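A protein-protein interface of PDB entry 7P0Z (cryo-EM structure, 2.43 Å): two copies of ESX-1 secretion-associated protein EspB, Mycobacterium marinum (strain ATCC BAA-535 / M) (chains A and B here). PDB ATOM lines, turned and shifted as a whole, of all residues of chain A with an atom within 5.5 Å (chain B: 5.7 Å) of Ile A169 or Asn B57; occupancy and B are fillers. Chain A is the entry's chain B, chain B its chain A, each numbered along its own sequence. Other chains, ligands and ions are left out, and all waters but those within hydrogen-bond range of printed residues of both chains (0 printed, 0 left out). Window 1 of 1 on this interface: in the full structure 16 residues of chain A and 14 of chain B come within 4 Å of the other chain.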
ATOM      1  N   LEU A 165      -5.672  -9.049  -3.407  1.00  0.00           N
ATOM      2  CA  LEU A 165      -4.459  -9.707  -2.947  1.00  0.00           C
ATOM      3  C   LEU A 165      -3.296  -8.738  -2.919  1.00  0.00           C
ATOM      4  O   LEU A 165      -2.534  -8.700  -1.955  1.00  0.00           O
ATOM      5  CB  LEU A 165      -4.110 -10.890  -3.834  1.00  0.00           C
ATOM      6  CG  LEU A 165      -4.904 -12.178  -3.750  1.00  0.00           C
ATOM      7  CD1 LEU A 165      -4.266 -13.190  -4.677  1.00  0.00           C
ATOM      8  CD2 LEU A 165      -4.934 -12.687  -2.343  1.00  0.00           C
ATOM      9  N   GLN A 166      -3.139  -7.950  -3.977  1.00  0.00           N
ATOM     10  CA  GLN A 166      -2.059  -6.976  -3.996  1.00  0.00           C
ATOM     11  C   GLN A 166      -2.156  -5.976  -2.855  1.00  0.00           C
ATOM     12  O   GLN A 166      -1.133  -5.502  -2.365  1.00  0.00           O
ATOM     13  CB  GLN A 166      -2.041  -6.248  -5.323  1.00  0.00           C
ATOM     14  CG  GLN A 166      -1.208  -6.908  -6.354  1.00  0.00           C
ATOM     15  CD  GLN A 166      -1.435  -6.351  -7.727  1.00  0.00           C
ATOM     16  OE1 GLN A 166      -0.512  -5.901  -8.368  1.00  0.00           O
ATOM     17  NE2 GLN A 166      -2.653  -6.430  -8.206  1.00  0.00           N
ATOM     18  N   ARG A 167      -3.353  -5.650  -2.414  1.00  0.00           N
ATOM     19  CA  ARG A 167      -3.458  -4.692  -1.330  1.00  0.00           C
ATOM     20  C   ARG A 167      -3.153  -5.290   0.022  1.00  0.00           C
ATOM     21  O   ARG A 167      -3.162  -4.562   1.010  1.00  0.00           O
ATOM     22  CB  ARG A 167      -4.845  -4.106  -1.225  1.00  0.00           C
ATOM     23  CG  ARG A 167      -5.274  -3.317  -2.356  1.00  0.00           C
ATOM     24  CD  ARG A 167      -6.616  -2.796  -2.054  1.00  0.00           C
ATOM     25  NE  ARG A 167      -7.118  -2.111  -3.212  1.00  0.00           N
ATOM     26  CZ  ARG A 167      -7.879  -2.704  -4.112  1.00  0.00           C
ATOM     27  NH1 ARG A 167      -8.256  -3.946  -3.917  1.00  0.00           N
ATOM     28  NH2 ARG A 167      -8.293  -2.046  -5.174  1.00  0.00           N
ATOM     29  N   ASP A 168      -2.925  -6.583   0.108  1.00  0.00           N
ATOM     30  CA  ASP A 168      -2.883  -7.246   1.392  1.00  0.00           C
ATOM     31  C   ASP A 168      -1.509  -7.802   1.722  1.00  0.00           C
ATOM     32  O   ASP A 168      -1.395  -8.783   2.443  1.00  0.00           O
ATOM     33  CB  ASP A 168      -3.930  -8.345   1.444  1.00  0.00           C
ATOM     34  CG  ASP A 168      -4.485  -8.530   2.814  1.00  0.00           C
ATOM     35  OD1 ASP A 168      -4.089  -7.772   3.715  1.00  0.00           O
ATOM     36  OD2 ASP A 168      -5.316  -9.433   3.008  1.00  0.00           O
ATOM     37  N   ILE A 169      -0.449  -7.173   1.233  1.00  0.00           N
ATOM     38  CA  ILE A 169       0.890  -7.609   1.578  1.00  0.00           C
ATOM     39  C   ILE A 169       1.502  -6.772   2.691  1.00  0.00           C
ATOM     40  O   ILE A 169       2.661  -6.975   3.030  1.00  0.00           O
ATOM     41  CB  ILE A 169       1.799  -7.633   0.345  1.00  0.00           C
ATOM     42  CG1 ILE A 169       1.896  -6.247  -0.268  1.00  0.00           C
ATOM     43  CG2 ILE A 169       1.305  -8.635  -0.652  1.00  0.00           C
ATOM     44  CD1 ILE A 169       3.050  -6.093  -1.158  1.00  0.00           C
ATOM     45  N   LYS A 170       0.752  -5.836   3.269  1.00  0.00           N
ATOM     46  CA  LYS A 170       1.212  -5.174   4.484  1.00  0.00           C
ATOM     47  C   LYS A 170       1.537  -6.170   5.568  1.00  0.00           C
ATOM     48  O   LYS A 170       2.473  -5.965   6.339  1.00  0.00           O
ATOM     49  CB  LYS A 170       0.156  -4.232   5.026  1.00  0.00           C
ATOM     50  CG  LYS A 170      -0.042  -3.003   4.270  1.00  0.00           C
ATOM     51  CD  LYS A 170      -1.315  -2.398   4.742  1.00  0.00           C
ATOM     52  CE  LYS A 170      -1.187  -2.006   6.182  1.00  0.00           C
ATOM     53  NZ  LYS A 170      -2.409  -1.314   6.659  1.00  0.00           N
ATOM     54  N   ARG A 171       0.769  -7.245   5.657  1.00  0.00           N
ATOM     55  CA  ARG A 171       0.977  -8.214   6.710  1.00  0.00           C
ATOM     56  C   ARG A 171       2.338  -8.880   6.647  1.00  0.00           C
ATOM     57  O   ARG A 171       2.659  -9.654   7.542  1.00  0.00           O
ATOM     58  CB  ARG A 171      -0.111  -9.274   6.664  1.00  0.00           C
ATOM     59  CG  ARG A 171      -0.094 -10.082   5.406  1.00  0.00           C
ATOM     60  CD  ARG A 171      -1.165 -11.125   5.425  1.00  0.00           C
ATOM     61  NE  ARG A 171      -2.509 -10.578   5.310  1.00  0.00           N
ATOM     62  CZ  ARG A 171      -3.596 -11.206   5.732  1.00  0.00           C
ATOM     63  NH1 ARG A 171      -3.491 -12.390   6.300  1.00  0.00           N
ATOM     64  NH2 ARG A 171      -4.782 -10.656   5.590  1.00  0.00           N
ATOM     65  N   PHE A 172       3.150  -8.612   5.637  1.00  0.00           N
ATOM     66  CA  PHE A 172       4.475  -9.200   5.578  1.00  0.00           C
ATOM     67  C   PHE A 172       5.584  -8.181   5.718  1.00  0.00           C
ATOM     68  O   PHE A 172       6.735  -8.511   5.458  1.00  0.00           O
ATOM     69  CB  PHE A 172       4.675  -9.967   4.283  1.00  0.00           C
ATOM     70  CG  PHE A 172       3.641 -10.967   4.021  1.00  0.00           C
ATOM     71  CD1 PHE A 172       3.465 -12.026   4.869  1.00  0.00           C
ATOM     72  CD2 PHE A 172       2.851 -10.870   2.913  1.00  0.00           C
ATOM     73  CE1 PHE A 172       2.512 -12.958   4.623  1.00  0.00           C
ATOM     74  CE2 PHE A 172       1.903 -11.809   2.657  1.00  0.00           C
ATOM     75  CZ  PHE A 172       1.735 -12.862   3.516  1.00  0.00           C
ATOM     76  N   ARG A 173       5.272  -6.961   6.116  1.00  0.00           N
ATOM     77  CA  ARG A 173       6.304  -5.957   6.278  1.00  0.00           C
ATOM     78  C   ARG A 173       7.288  -6.357   7.367  1.00  0.00           C
ATOM     79  O   ARG A 173       7.007  -7.188   8.225  1.00  0.00           O
ATOM     80  CB  ARG A 173       5.680  -4.616   6.613  1.00  0.00           C
ATOM     81  CG  ARG A 173       5.098  -4.574   7.963  1.00  0.00           C
ATOM     82  CD  ARG A 173       4.311  -3.338   8.152  1.00  0.00           C
ATOM     83  NE  ARG A 173       3.697  -3.325   9.462  1.00  0.00           N
ATOM     84  CZ  ARG A 173       2.573  -3.949   9.755  1.00  0.00           C
ATOM     85  NH1 ARG A 173       1.956  -4.654   8.833  1.00  0.00           N
ATOM     86  NH2 ARG A 173       2.076  -3.883  10.968  1.00  0.00           N
ATOM     87  N   LYS A 194       5.119 -13.291   0.877  1.00  0.00           N
ATOM     88  CA  LYS A 194       4.736 -12.147   0.074  1.00  0.00           C
ATOM     89  C   LYS A 194       4.984 -12.417  -1.402  1.00  0.00           C
ATOM     90  O   LYS A 194       4.149 -12.092  -2.252  1.00  0.00           O
ATOM     91  CB  LYS A 194       5.523 -10.933   0.548  1.00  0.00           C
ATOM     92  CG  LYS A 194       5.102  -9.592   0.017  1.00  0.00           C
ATOM     93  CD  LYS A 194       5.773  -9.306  -1.274  1.00  0.00           C
ATOM     94  CE  LYS A 194       7.243  -9.314  -1.086  1.00  0.00           C
ATOM     95  NZ  LYS A 194       7.934  -8.996  -2.345  1.00  0.00           N
ATOM     96  N   ILE A 197       2.343 -14.715  -2.694  1.00  0.00           N
ATOM     97  CA  ILE A 197       1.069 -14.029  -2.838  1.00  0.00           C
ATOM     98  C   ILE A 197       1.055 -13.176  -4.099  1.00  0.00           C
ATOM     99  O   ILE A 197       0.053 -13.117  -4.810  1.00  0.00           O
ATOM    100  CB  ILE A 197       0.772 -13.199  -1.577  1.00  0.00           C
ATOM    101  CG1 ILE A 197       0.407 -14.114  -0.424  1.00  0.00           C
ATOM    102  CG2 ILE A 197      -0.343 -12.211  -1.819  1.00  0.00           C
ATOM    103  CD1 ILE A 197      -0.926 -14.718  -0.554  1.00  0.00           C
ATOM    104  N   LEU A 198       2.153 -12.492  -4.387  1.00  0.00           N
ATOM    105  CA  LEU A 198       2.197 -11.692  -5.602  1.00  0.00           C
ATOM    106  C   LEU A 198       2.124 -12.566  -6.843  1.00  0.00           C
ATOM    107  O   LEU A 198       1.457 -12.216  -7.819  1.00  0.00           O
ATOM    108  CB  LEU A 198       3.451 -10.837  -5.613  1.00  0.00           C
ATOM    109  CG  LEU A 198       3.316  -9.660  -4.662  1.00  0.00           C
ATOM    110  CD1 LEU A 198       4.429  -8.698  -4.861  1.00  0.00           C
ATOM    111  CD2 LEU A 198       2.004  -8.976  -4.885  1.00  0.00           C
ATOM    112  N   ALA B  52      -2.591   2.789  -8.135  1.00  0.00           N
ATOM    113  CA  ALA B  52      -2.629   3.144  -6.727  1.00  0.00           C
ATOM    114  C   ALA B  52      -1.961   2.077  -5.877  1.00  0.00           C
ATOM    115  O   ALA B  52      -1.192   2.388  -4.961  1.00  0.00           O
ATOM    116  CB  ALA B  52      -4.067   3.368  -6.284  1.00  0.00           C
ATOM    117  N   VAL B  53      -2.223   0.812  -6.184  1.00  0.00           N
ATOM    118  CA  VAL B  53      -1.632  -0.271  -5.417  1.00  0.00           C
ATOM    119  C   VAL B  53      -0.127  -0.313  -5.613  1.00  0.00           C
ATOM    120  O   VAL B  53       0.630  -0.507  -4.656  1.00  0.00           O
ATOM    121  CB  VAL B  53      -2.293  -1.608  -5.788  1.00  0.00           C
ATOM    122  CG1 VAL B  53      -1.657  -2.723  -5.032  1.00  0.00           C
ATOM    123  CG2 VAL B  53      -3.743  -1.568  -5.436  1.00  0.00           C
ATOM    124  N   SER B  54       0.335  -0.138  -6.842  1.00  0.00           N
ATOM    125  CA  SER B  54       1.767  -0.121  -7.085  1.00  0.00           C
ATOM    126  C   SER B  54       2.440   1.020  -6.339  1.00  0.00           C
ATOM    127  O   SER B  54       3.533   0.853  -5.790  1.00  0.00           O
ATOM    128  CB  SER B  54       2.038  -0.015  -8.574  1.00  0.00           C
ATOM    129  OG  SER B  54       1.935  -1.270  -9.190  1.00  0.00           O
ATOM    130  N   ALA B  55       1.802   2.186  -6.306  1.00  0.00           N
ATOM    131  CA  ALA B  55       2.366   3.305  -5.571  1.00  0.00           C
ATOM    132  C   ALA B  55       2.466   3.001  -4.085  1.00  0.00           C
ATOM    133  O   ALA B  55       3.495   3.272  -3.456  1.00  0.00           O
ATOM    134  CB  ALA B  55       1.531   4.556  -5.805  1.00  0.00           C
ATOM    135  N   ASP B  56       1.406   2.444  -3.509  1.00  0.00           N
ATOM    136  CA  ASP B  56       1.449   2.045  -2.109  1.00  0.00           C
ATOM    137  C   ASP B  56       2.578   1.060  -1.839  1.00  0.00           C
ATOM    138  O   ASP B  56       3.281   1.166  -0.828  1.00  0.00           O
ATOM    139  CB  ASP B  56       0.117   1.437  -1.701  1.00  0.00           C
ATOM    140  CG  ASP B  56      -0.920   2.473  -1.410  1.00  0.00           C
ATOM    141  OD1 ASP B  56      -0.547   3.560  -0.945  1.00  0.00           O
ATOM    142  OD2 ASP B  56      -2.110   2.214  -1.649  1.00  0.00           O
ATOM    143  N   ASN B  57       2.766   0.101  -2.726  1.00  0.00           N
ATOM    144  CA  ASN B  57       3.788  -0.901  -2.487  1.00  0.00           C
ATOM    145  C   ASN B  57       5.182  -0.302  -2.567  1.00  0.00           C
ATOM    146  O   ASN B  57       6.071  -0.660  -1.782  1.00  0.00           O
ATOM    147  CB  ASN B  57       3.594  -2.046  -3.471  1.00  0.00           C
ATOM    148  CG  ASN B  57       2.420  -2.915  -3.095  1.00  0.00           C
ATOM    149  OD1 ASN B  57       1.649  -2.574  -2.208  1.00  0.00           O
ATOM    150  ND2 ASN B  57       2.257  -4.026  -3.786  1.00  0.00           N
ATOM    151  N   VAL B  58       5.384   0.630  -3.486  1.00  0.00           N
ATOM    152  CA  VAL B  58       6.669   1.301  -3.572  1.00  0.00           C
ATOM    153  C   VAL B  58       6.935   2.118  -2.312  1.00  0.00           C
ATOM    154  O   VAL B  58       8.050   2.119  -1.782  1.00  0.00           O
ATOM    155  CB  VAL B  58       6.731   2.159  -4.843  1.00  0.00           C
ATOM    156  CG1 VAL B  58       7.866   3.152  -4.767  1.00  0.00           C
ATOM    157  CG2 VAL B  58       6.874   1.279  -6.051  1.00  0.00           C
ATOM    158  N   ARG B  59       5.919   2.807  -1.803  1.00  0.00           N
ATOM    159  CA  ARG B  59       6.115   3.584  -0.585  1.00  0.00           C
ATOM    160  C   ARG B  59       6.486   2.688   0.592  1.00  0.00           C
ATOM    161  O   ARG B  59       7.363   3.024   1.403  1.00  0.00           O
ATOM    162  CB  ARG B  59       4.861   4.401  -0.281  1.00  0.00           C
ATOM    163  CG  ARG B  59       4.744   5.634  -1.136  1.00  0.00           C
ATOM    164  CD  ARG B  59       3.596   6.517  -0.743  1.00  0.00           C
ATOM    165  NE  ARG B  59       2.317   5.900  -1.045  1.00  0.00           N
ATOM    166  CZ  ARG B  59       1.584   6.173  -2.114  1.00  0.00           C
ATOM    167  NH1 ARG B  59       1.983   7.063  -2.998  1.00  0.00           N
ATOM    168  NH2 ARG B  59       0.444   5.550  -2.292  1.00  0.00           N
ATOM    169  N   LEU B  60       5.841   1.531   0.682  1.00  0.00           N
ATOM    170  CA  LEU B  60       6.160   0.574   1.727  1.00  0.00           C
ATOM    171  C   LEU B  60       7.617   0.126   1.664  1.00  0.00           C
ATOM    172  O   LEU B  60       8.329   0.094   2.681  1.00  0.00           O
ATOM    173  CB  LEU B  60       5.230  -0.613   1.589  1.00  0.00           C
ATOM    174  CG  LEU B  60       5.289  -1.632   2.702  1.00  0.00           C
ATOM    175  CD1 LEU B  60       4.550  -1.096   3.889  1.00  0.00           C
ATOM    176  CD2 LEU B  60       4.677  -2.895   2.207  1.00  0.00           C
ATOM    177  N   TYR B  61       8.087  -0.223   0.480  1.00  0.00           N
ATOM    178  CA  TYR B  61       9.474  -0.652   0.405  1.00  0.00           C
ATOM    179  C   TYR B  61      10.445   0.490   0.663  1.00  0.00           C
ATOM    180  O   TYR B  61      11.573   0.257   1.105  1.00  0.00           O
ATOM    181  CB  TYR B  61       9.746  -1.297  -0.931  1.00  0.00           C
ATOM    182  CG  TYR B  61       9.370  -2.717  -0.879  1.00  0.00           C
ATOM    183  CD1 TYR B  61       8.072  -3.101  -1.107  1.00  0.00           C
ATOM    184  CD2 TYR B  61      10.295  -3.682  -0.545  1.00  0.00           C
ATOM    185  CE1 TYR B  61       7.710  -4.386  -1.039  1.00  0.00           C
ATOM    186  CE2 TYR B  61       9.940  -4.979  -0.469  1.00  0.00           C
ATOM    187  CZ  TYR B  61       8.648  -5.327  -0.722  1.00  0.00           C
ATOM    188  OH  TYR B  61       8.277  -6.629  -0.650  1.00  0.00           O
ATOM    189  N   LEU B  62      10.040   1.721   0.392  1.00  0.00           N
ATOM    190  CA  LEU B  62      10.899   2.835   0.742  1.00  0.00           C
ATOM    191  C   LEU B  62      11.074   2.929   2.246  1.00  0.00           C
ATOM    192  O   LEU B  62      12.169   3.218   2.735  1.00  0.00           O
ATOM    193  CB  LEU B  62      10.332   4.124   0.180  1.00  0.00           C
ATOM    194  CG  LEU B  62      10.523   4.206  -1.323  1.00  0.00           C
ATOM    195  CD1 LEU B  62       9.731   5.348  -1.849  1.00  0.00           C
ATOM    196  CD2 LEU B  62      11.971   4.312  -1.711  1.00  0.00           C
ATOM    197  N   VAL B 274       3.918  -3.640 -10.036  1.00  0.00           N
ATOM    198  CA  VAL B 274       5.296  -3.288  -9.736  1.00  0.00           C
ATOM    199  C   VAL B 274       5.633  -3.894  -8.391  1.00  0.00           C
ATOM    200  O   VAL B 274       5.088  -3.459  -7.379  1.00  0.00           O
ATOM    201  CB  VAL B 274       5.492  -1.768  -9.704  1.00  0.00           C
ATOM    202  CG1 VAL B 274       6.919  -1.421  -9.385  1.00  0.00           C
ATOM    203  CG2 VAL B 274       5.099  -1.171 -11.014  1.00  0.00           C
ATOM    204  N   PRO B 276       8.571  -4.200  -5.721  1.00  0.00           N
ATOM    205  CA  PRO B 276       9.911  -3.770  -5.366  1.00  0.00           C
ATOM    206  C   PRO B 276      10.659  -4.873  -4.653  1.00  0.00           C
ATOM    207  O   PRO B 276      10.083  -5.576  -3.816  1.00  0.00           O
ATOM    208  CB  PRO B 276       9.659  -2.591  -4.422  1.00  0.00           C
ATOM    209  CG  PRO B 276       8.200  -2.340  -4.480  1.00  0.00           C
ATOM    210  CD  PRO B 276       7.553  -3.588  -4.867  1.00  0.00           C
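The side-chain hydroxyl (OH) of Tyr B61 sits close to the side-chain amino group (NZ) of Lys A194 (2.9 Å).
O of Val B53 sits close to OD1 of Asn B57 (3.4 Å).
Gln A166 touches Val B53. Asn B57 touches Gln A166 (ND2 to O, 3.96 Å). CG2 of Val B53 touches CG of Arg A167, 3.9 Å away. CD1 of Ile A169 touches ND2 of Asn B57 (3.4 Å).
Of the printed residues of chain B, Gln A166 touches Val B53 and Asn B57. Printed residues of chain B within 4 Å of Arg A167: Val B53 (3.9 Å). Ile A169 touches just one residue of chain B: Asn B57 (3.4 Å). Phe A172 touches none of the printed residues of chain B. Of chain A, only Gln A166 (3.96 Å) and Ile A169 (3.4 Å) come within 4 Å of Asn B57. Leu B60 touches none of the printed residues of chain A. Of the printed residues of chain A, Tyr B61 touches Lys A194. The nearest residue of chain B that does not touch Ile A169 is Leu B60 (4.6 Å). The nearest residue of chain A that does not touch Asn B57 is Leu A198 (5.1 Å). The nearest printed residue of chain B that does not touch Lys A194 is Pro B276 (4.3 Å).
Of the 13 printed residues of chain B, 3 touch a printed residue of chain A. Printed residues of chain B that touch a printed residue of chain A: Val B53, Asn B57 and Tyr B61. Hydrophobic or aromatic side chains of chain B that line the printed part of chain A: Val B53 and Tyr B61. Along chain B the printed residues that touch a printed residue of chain A span positions 53 to 61. Of the 12 printed residues of chain A, 4 touch a printed residue of chain B. Printed residues of chain A that touch a printed residue of chain B: Gln A166, Arg A167, Ile A169 and Lys A194. Hydrophobic or aromatic side chains of chain A that line the printed part of chain B: Ile A169. Along chain A the printed residues that touch a printed residue of chain B span positions 166 to 194. Among the printed residues, 5 pairs touch across the chains.
No position is printed for both chains.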
